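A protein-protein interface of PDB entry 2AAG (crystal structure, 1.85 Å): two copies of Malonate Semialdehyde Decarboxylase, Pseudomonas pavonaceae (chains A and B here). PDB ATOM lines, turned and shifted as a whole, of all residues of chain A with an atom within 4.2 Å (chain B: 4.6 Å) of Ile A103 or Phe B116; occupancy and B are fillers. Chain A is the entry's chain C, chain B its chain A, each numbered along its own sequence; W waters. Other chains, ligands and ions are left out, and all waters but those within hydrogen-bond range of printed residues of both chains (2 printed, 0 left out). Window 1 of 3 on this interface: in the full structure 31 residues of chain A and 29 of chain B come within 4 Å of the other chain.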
ATOM      1  N   LEU A  52      14.430 -13.121 -17.765  1.00  0.00           N
ATOM      2  CA  LEU A  52      14.915 -13.136 -19.141  1.00  0.00           C
ATOM      3  C   LEU A  52      13.900 -13.964 -19.920  1.00  0.00           C
ATOM      4  O   LEU A  52      13.847 -15.170 -19.710  1.00  0.00           O
ATOM      5  CB  LEU A  52      16.334 -13.738 -19.214  1.00  0.00           C
ATOM      6  CG  LEU A  52      17.419 -12.904 -18.440  1.00  0.00           C
ATOM      7  CD1 LEU A  52      18.709 -13.683 -18.122  1.00  0.00           C
ATOM      8  CD2 LEU A  52      17.681 -11.534 -19.034  1.00  0.00           C
ATOM      9  N   LEU A  57      10.213 -15.974 -29.317  1.00  0.00           N
ATOM     10  CA  LEU A  57      11.006 -16.700 -30.271  1.00  0.00           C
ATOM     11  C   LEU A  57      11.055 -18.193 -30.045  1.00  0.00           C
ATOM     12  O   LEU A  57      11.615 -18.869 -30.906  1.00  0.00           O
ATOM     13  CB  LEU A  57      12.450 -16.162 -30.374  1.00  0.00           C
ATOM     14  CG  LEU A  57      12.555 -14.765 -30.971  1.00  0.00           C
ATOM     15  CD1 LEU A  57      13.881 -14.065 -30.553  1.00  0.00           C
ATOM     16  CD2 LEU A  57      12.390 -14.723 -32.446  1.00  0.00           C
ATOM     17  N   TYR A  59      12.520 -19.955 -27.094  1.00  0.00           N
ATOM     18  CA  TYR A  59      13.747 -20.373 -26.407  1.00  0.00           C
ATOM     19  C   TYR A  59      13.252 -20.609 -24.945  1.00  0.00           C
ATOM     20  O   TYR A  59      12.693 -19.712 -24.424  1.00  0.00           O
ATOM     21  CB  TYR A  59      14.714 -19.156 -26.459  1.00  0.00           C
ATOM     22  CG  TYR A  59      15.125 -18.624 -27.844  1.00  0.00           C
ATOM     23  CD1 TYR A  59      15.078 -19.415 -28.978  1.00  0.00           C
ATOM     24  CD2 TYR A  59      15.551 -17.286 -27.991  1.00  0.00           C
ATOM     25  CE1 TYR A  59      15.489 -18.886 -30.256  1.00  0.00           C
ATOM     26  CE2 TYR A  59      15.962 -16.781 -29.192  1.00  0.00           C
ATOM     27  CZ  TYR A  59      15.925 -17.576 -30.334  1.00  0.00           C
ATOM     28  OH  TYR A  59      16.293 -17.048 -31.568  1.00  0.00           O
ATOM     29  N   ARG A  61      14.725 -21.218 -21.653  1.00  0.00           N
ATOM     30  CA  ARG A  61      15.667 -20.684 -20.594  1.00  0.00           C
ATOM     31  C   ARG A  61      15.710 -21.455 -19.288  1.00  0.00           C
ATOM     32  O   ARG A  61      14.651 -21.732 -18.714  1.00  0.00           O
ATOM     33  CB  ARG A  61      15.441 -19.185 -20.226  1.00  0.00           C
ATOM     34  CG  ARG A  61      14.862 -18.323 -21.287  1.00  0.00           C
ATOM     35  CD  ARG A  61      15.953 -17.716 -22.039  1.00  0.00           C
ATOM     36  NE  ARG A  61      15.650 -16.658 -22.947  1.00  0.00           N
ATOM     37  CZ  ARG A  61      16.319 -16.381 -24.026  1.00  0.00           C
ATOM     38  NH1 ARG A  61      17.218 -17.059 -24.500  1.00  0.00           N
ATOM     39  NH2 ARG A  61      16.079 -15.396 -24.762  1.00  0.00           N
ATOM     40  N   VAL A  65      21.120 -19.908 -17.636  1.00  0.00           N
ATOM     41  CA  VAL A  65      21.117 -18.813 -18.620  1.00  0.00           C
ATOM     42  C   VAL A  65      22.229 -17.763 -18.378  1.00  0.00           C
ATOM     43  O   VAL A  65      22.495 -17.363 -17.211  1.00  0.00           O
ATOM     44  CB  VAL A  65      19.762 -18.125 -18.666  1.00  0.00           C
ATOM     45  CG1 VAL A  65      19.548 -17.215 -17.506  1.00  0.00           C
ATOM     46  CG2 VAL A  65      19.706 -17.170 -19.720  1.00  0.00           C
ATOM     47  N   VAL A  66      22.854 -17.360 -19.474  1.00  0.00           N
ATOM     48  CA  VAL A  66      23.950 -16.386 -19.424  1.00  0.00           C
ATOM     49  C   VAL A  66      23.533 -15.158 -20.217  1.00  0.00           C
ATOM     50  O   VAL A  66      23.147 -15.248 -21.407  1.00  0.00           O
ATOM     51  CB  VAL A  66      25.253 -16.953 -20.117  1.00  0.00           C
ATOM     52  CG1 VAL A  66      26.442 -15.897 -20.105  1.00  0.00           C
ATOM     53  CG2 VAL A  66      25.706 -18.310 -19.496  1.00  0.00           C
ATOM     54  N   LEU A  67      23.596 -13.984 -19.582  1.00  0.00           N
ATOM     55  CA  LEU A  67      23.361 -12.727 -20.272  1.00  0.00           C
ATOM     56  C   LEU A  67      24.722 -12.047 -20.395  1.00  0.00           C
ATOM     57  O   LEU A  67      25.402 -11.821 -19.376  1.00  0.00           O
ATOM     58  CB  LEU A  67      22.409 -11.853 -19.469  1.00  0.00           C
ATOM     59  CG  LEU A  67      22.287 -10.415 -19.977  1.00  0.00           C
ATOM     60  CD1 LEU A  67      21.672 -10.290 -21.354  1.00  0.00           C
ATOM     61  CD2 LEU A  67      21.531  -9.602 -18.912  1.00  0.00           C
ATOM     62  N   LEU A  68      25.145 -11.762 -21.602  1.00  0.00           N
ATOM     63  CA  LEU A  68      26.459 -11.160 -21.772  1.00  0.00           C
ATOM     64  C   LEU A  68      26.247  -9.795 -22.368  1.00  0.00           C
ATOM     65  O   LEU A  68      25.585  -9.689 -23.388  1.00  0.00           O
ATOM     66  CB  LEU A  68      27.289 -11.979 -22.764  1.00  0.00           C
ATOM     67  CG  LEU A  68      28.579 -11.345 -23.301  1.00  0.00           C
ATOM     68  CD1 LEU A  68      29.512 -11.132 -22.114  1.00  0.00           C
ATOM     69  CD2 LEU A  68      29.184 -12.376 -24.294  1.00  0.00           C
ATOM     70  N   VAL A 102      21.769 -18.563 -23.990  1.00  0.00           N
ATOM     71  CA  VAL A 102      22.755 -17.474 -24.254  1.00  0.00           C
ATOM     72  C   VAL A 102      22.114 -16.211 -24.862  1.00  0.00           C
ATOM     73  O   VAL A 102      21.603 -16.238 -25.955  1.00  0.00           O
ATOM     74  CB  VAL A 102      23.930 -17.971 -25.151  1.00  0.00           C
ATOM     75  CG1 VAL A 102      24.967 -16.880 -25.263  1.00  0.00           C
ATOM     76  CG2 VAL A 102      24.613 -19.189 -24.466  1.00  0.00           C
ATOM     77  N   ILE A 103      22.209 -15.064 -24.163  1.00  0.00           N
ATOM     78  CA  ILE A 103      21.669 -13.788 -24.661  1.00  0.00           C
ATOM     79  C   ILE A 103      22.810 -12.716 -24.656  1.00  0.00           C
ATOM     80  O   ILE A 103      23.629 -12.717 -23.716  1.00  0.00           O
ATOM     81  CB  ILE A 103      20.566 -13.307 -23.685  1.00  0.00           C
ATOM     82  CG1 ILE A 103      19.442 -14.346 -23.577  1.00  0.00           C
ATOM     83  CG2 ILE A 103      20.040 -11.899 -24.121  1.00  0.00           C
ATOM     84  CD1 ILE A 103      18.532 -14.101 -22.240  1.00  0.00           C
ATOM     85  N   VAL A 104      22.970 -12.005 -25.768  1.00  0.00           N
ATOM     86  CA  VAL A 104      24.070 -11.054 -25.959  1.00  0.00           C
ATOM     87  C   VAL A 104      23.493  -9.708 -26.358  1.00  0.00           C
ATOM     88  O   VAL A 104      22.682  -9.619 -27.288  1.00  0.00           O
ATOM     89  CB  VAL A 104      25.041 -11.506 -27.044  1.00  0.00           C
ATOM     90  CG1 VAL A 104      26.276 -10.563 -27.090  1.00  0.00           C
ATOM     91  CG2 VAL A 104      25.438 -12.939 -26.826  1.00  0.00           C
ATOM     92  N   TYR B  39      13.850  -8.384 -20.550  1.00  0.00           N
ATOM     93  CA  TYR B  39      15.207  -8.746 -20.181  1.00  0.00           C
ATOM     94  C   TYR B  39      15.608  -7.746 -19.088  1.00  0.00           C
ATOM     95  O   TYR B  39      15.708  -6.549 -19.406  1.00  0.00           O
ATOM     96  CB  TYR B  39      16.135  -8.571 -21.409  1.00  0.00           C
ATOM     97  CG  TYR B  39      15.659  -9.494 -22.506  1.00  0.00           C
ATOM     98  CD1 TYR B  39      16.059 -10.779 -22.564  1.00  0.00           C
ATOM     99  CD2 TYR B  39      14.751  -9.066 -23.448  1.00  0.00           C
ATOM    100  CE1 TYR B  39      15.569 -11.698 -23.605  1.00  0.00           C
ATOM    101  CE2 TYR B  39      14.247  -9.977 -24.448  1.00  0.00           C
ATOM    102  CZ  TYR B  39      14.661 -11.273 -24.515  1.00  0.00           C
ATOM    103  OH  TYR B  39      14.153 -12.094 -25.530  1.00  0.00           O
ATOM    104  N   TRP B 114      22.258  -7.510 -31.110  1.00  0.00           N
ATOM    105  CA  TRP B 114      21.459  -8.343 -30.243  1.00  0.00           C
ATOM    106  C   TRP B 114      21.452  -9.763 -30.701  1.00  0.00           C
ATOM    107  O   TRP B 114      21.316 -10.019 -31.901  1.00  0.00           O
ATOM    108  CB  TRP B 114      19.966  -7.894 -30.148  1.00  0.00           C
ATOM    109  CG  TRP B 114      19.781  -6.510 -29.643  1.00  0.00           C
ATOM    110  CD1 TRP B 114      19.811  -5.347 -30.343  1.00  0.00           C
ATOM    111  CD2 TRP B 114      19.630  -6.165 -28.291  1.00  0.00           C
ATOM    112  NE1 TRP B 114      19.636  -4.282 -29.486  1.00  0.00           N
ATOM    113  CE2 TRP B 114      19.500  -4.758 -28.214  1.00  0.00           C
ATOM    114  CE3 TRP B 114      19.539  -6.911 -27.120  1.00  0.00           C
ATOM    115  CZ2 TRP B 114      19.326  -4.059 -26.978  1.00  0.00           C
ATOM    116  CZ3 TRP B 114      19.333  -6.222 -25.870  1.00  0.00           C
ATOM    117  CH2 TRP B 114      19.252  -4.809 -25.839  1.00  0.00           C
ATOM    118  N   SER B 115      21.621 -10.692 -29.758  1.00  0.00           N
ATOM    119  CA  SER B 115      21.374 -12.072 -30.056  1.00  0.00           C
ATOM    120  C   SER B 115      20.546 -12.646 -28.946  1.00  0.00           C
ATOM    121  O   SER B 115      21.075 -12.772 -27.795  1.00  0.00           O
ATOM    122  CB  SER B 115      22.689 -12.846 -30.209  1.00  0.00           C
ATOM    123  OG  SER B 115      22.403 -14.223 -30.396  1.00  0.00           O
ATOM    124  N   PHE B 116      19.263 -12.981 -29.236  1.00  0.00           N
ATOM    125  CA  PHE B 116      18.402 -13.455 -28.169  1.00  0.00           C
ATOM    126  C   PHE B 116      18.493 -14.946 -27.800  1.00  0.00           C
ATOM    127  O   PHE B 116      18.019 -15.362 -26.743  1.00  0.00           O
ATOM    128  CB  PHE B 116      16.917 -13.015 -28.363  1.00  0.00           C
ATOM    129  CG  PHE B 116      16.772 -11.528 -28.360  1.00  0.00           C
ATOM    130  CD1 PHE B 116      16.876 -10.835 -27.175  1.00  0.00           C
ATOM    131  CD2 PHE B 116      16.670 -10.813 -29.558  1.00  0.00           C
ATOM    132  CE1 PHE B 116      16.806  -9.395 -27.152  1.00  0.00           C
ATOM    133  CE2 PHE B 116      16.635  -9.385 -29.539  1.00  0.00           C
ATOM    134  CZ  PHE B 116      16.677  -8.688 -28.322  1.00  0.00           C
ATOM    135  N   GLY B 117      19.071 -15.747 -28.689  1.00  0.00           N
ATOM    136  CA  GLY B 117      19.251 -17.139 -28.354  1.00  0.00           C
ATOM    137  C   GLY B 117      19.766 -17.845 -29.575  1.00  0.00           C
ATOM    138  O   GLY B 117      19.724 -17.266 -30.660  1.00  0.00           O
ATOM    139  N   ARG B 120      21.807 -16.524 -32.794  1.00  0.00           N
ATOM    140  CA  ARG B 120      21.107 -15.914 -33.955  1.00  0.00           C
ATOM    141  C   ARG B 120      21.047 -14.398 -33.762  1.00  0.00           C
ATOM    142  O   ARG B 120      21.025 -13.934 -32.596  1.00  0.00           O
ATOM    143  CB  ARG B 120      19.651 -16.479 -34.022  1.00  0.00           C
ATOM    144  CG  ARG B 120      19.566 -17.923 -34.461  1.00  0.00           C
ATOM    145  CD  ARG B 120      18.125 -18.453 -34.439  1.00  0.00           C
ATOM    146  NE  ARG B 120      18.163 -19.863 -34.795  1.00  0.00           N
ATOM    147  CZ  ARG B 120      17.123 -20.718 -34.747  1.00  0.00           C
ATOM    148  NH1 ARG B 120      15.912 -20.330 -34.323  1.00  0.00           N
ATOM    149  NH2 ARG B 120      17.316 -21.993 -35.120  1.00  0.00           N
ATOM    150  N   GLU B 122      18.498 -11.991 -34.365  1.00  0.00           N
ATOM    151  CA  GLU B 122      17.078 -11.998 -34.818  1.00  0.00           C
ATOM    152  C   GLU B 122      16.505 -10.735 -35.460  1.00  0.00           C
ATOM    153  O   GLU B 122      15.548 -10.838 -36.244  1.00  0.00           O
ATOM    154  CB  GLU B 122      16.163 -12.487 -33.698  1.00  0.00           C
ATOM    155  CG  GLU B 122      16.568 -13.845 -33.192  1.00  0.00           C
ATOM    156  CD  GLU B 122      17.494 -13.815 -31.956  1.00  0.00           C
ATOM    157  OE1 GLU B 122      18.196 -12.773 -31.653  1.00  0.00           O
ATOM    158  OE2 GLU B 122      17.545 -14.859 -31.271  1.00  0.00           O
ATOM    159  N   PHE B 123      17.041  -9.552 -35.147  1.00  0.00           N
ATOM    160  CA  PHE B 123      16.648  -8.364 -35.901  1.00  0.00           C
ATOM    161  C   PHE B 123      17.191  -8.405 -37.333  1.00  0.00           C
ATOM    162  O   PHE B 123      16.543  -7.894 -38.232  1.00  0.00           O
ATOM    163  CB  PHE B 123      17.068  -7.059 -35.205  1.00  0.00           C
ATOM    164  CG  PHE B 123      16.455  -6.883 -33.862  1.00  0.00           C
ATOM    165  CD1 PHE B 123      15.079  -6.941 -33.707  1.00  0.00           C
ATOM    166  CD2 PHE B 123      17.247  -6.652 -32.730  1.00  0.00           C
ATOM    167  CE1 PHE B 123      14.481  -6.776 -32.399  1.00  0.00           C
ATOM    168  CE2 PHE B 123      16.651  -6.464 -31.425  1.00  0.00           C
ATOM    169  CZ  PHE B 123      15.262  -6.515 -31.288  1.00  0.00           C
ATOM    170  N   LEU B 128      12.558 -11.049 -35.690  1.00  0.00           N
ATOM    171  CA  LEU B 128      11.998  -9.936 -34.925  1.00  0.00           C
ATOM    172  C   LEU B 128      11.977  -8.598 -35.714  1.00  0.00           C
ATOM    173  O   LEU B 128      12.876  -8.343 -36.513  1.00  0.00           O
ATOM    174  CB  LEU B 128      12.819  -9.712 -33.618  1.00  0.00           C
ATOM    175  CG  LEU B 128      12.706 -10.757 -32.526  1.00  0.00           C
ATOM    176  CD1 LEU B 128      13.595 -10.362 -31.356  1.00  0.00           C
ATOM    177  CD2 LEU B 128      11.223 -11.022 -32.027  1.00  0.00           C
HETATM  178  O   HOH W   1      22.522 -16.435 -28.563  1.00  0.00           O
HETATM  179  O   HOH W   2      14.951 -17.460 -33.925  1.00  0.00           O
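N of Val A104 is in hydrogen-bond range of O of Ser B115.
O of Phe B116 lies within hydrogen-bond range of NH2 of Arg A61 (2.8 Å).
The side-chain carboxylate (OE2) of Glu B122 lies within hydrogen-bond range of the side-chain hydroxyl (OH) of Tyr A59 (2.5 Å).
OG of Ser B115 sits at hydrogen-bond distance from O of Arg B120 (2.6 Å).
N of Phe B116 is in hydrogen-bond range of OE1 of Glu B122 (2.7 Å).
The side-chain carboxylate (OE2) of Glu B122 lies within hydrogen-bond range of the backbone NH (N) of Gly B117 (3.1 Å).
The backbone NH of Leu B128 sits at hydrogen-bond distance from the backbone carbonyl oxygen of Glu B122 (3.0 Å).
The backbone carbonyl oxygen (O) of Val A66 is in hydrogen-bond range of the backbone NH (N) of Ile A103 (2.9 Å).
The backbone NH of Leu A68 lies within hydrogen-bond range of the backbone carbonyl oxygen of Ile A103 (2.8 Å).
Among the printed residues, merely in contact across the chains: Tyr A59 with Gly B117 (3.3 Å), Ile A103 with Ser B115 (3.3 Å), Tyr A59 with Phe B116 (3.4 Å), Val A104 with Trp B114 (3.4 Å), Val A102 with Gly B117 (3.5 Å), Ile A103 with Phe B116 (3.6 Å), Tyr A59 with Arg B120 (3.7 Å), Leu A57 with Glu B122 (3.8 Å), Val A102 with Phe B116 (3.8 Å), Leu A57 with Leu B128 (3.8 Å), Leu A57 with Phe B116 (3.9 Å), Arg A61 with Tyr B39 (3.9 Å), Leu A52 with Tyr B39 (3.9 Å) and Val A102 with Ser B115 (3.96 Å).
Of the printed residues of chain B, Ile A103 touches Ser B115 and Phe B116.
Of chain A, only Leu A57 (3.9 Å), Tyr A59 (3.4 Å), Arg A61 (2.8 Å), Val A102 (3.8 Å) and Ile A103 (3.6 Å) come within 4 Å of Phe B116.
Printed residues of chain B within 4 Å of Arg A61: Tyr B39 (3.9 Å) and Phe B116 (2.8 Å).
Of the printed residues of chain A, Trp B114 touches Val A104.
Printed residues of chain B within 4 Å of Tyr A59: Phe B116 (3.4 Å), Gly B117 (3.3 Å), Arg B120 (3.7 Å) and Glu B122 (2.5 Å).
The nearest residue of chain B that does not touch Ile A103 is Tyr B39 (4.1 Å).
The nearest printed residue of chain A that does not touch Phe B116 is Val A104 (5.2 Å).
Of the 11 printed residues of chain A, 7 touch a printed residue of chain B.
Hydrophobic or aromatic side chains of chain A within 4 Å of the printed part of chain B: Leu A52, Leu A57, Tyr A59 and Ile A103.
Of the 9 printed residues of chain B, 8 touch a printed residue of chain A.
Hydrophobic or aromatic side chains of chain B that line the printed part of chain A: Tyr B39, Phe B116 and Leu B128.
Among the printed residues, 17 pairs touch across the chains.
No position is printed for both chains.
Of the 17 pairs that touch across the chains among the printed residues, none has its exchanged pair printed and touching as well.
Water W2 lies within hydrogen-bond range of the side-chain hydroxyl of Tyr A59 (2.7 Å) and the guanidinium group of Arg B120 (3.1 Å).
Water W1 bridges the backbone carbonyl oxygen of Val A102 (2.8 Å) and the side-chain hydroxyl of Ser B115 (2.9 Å).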
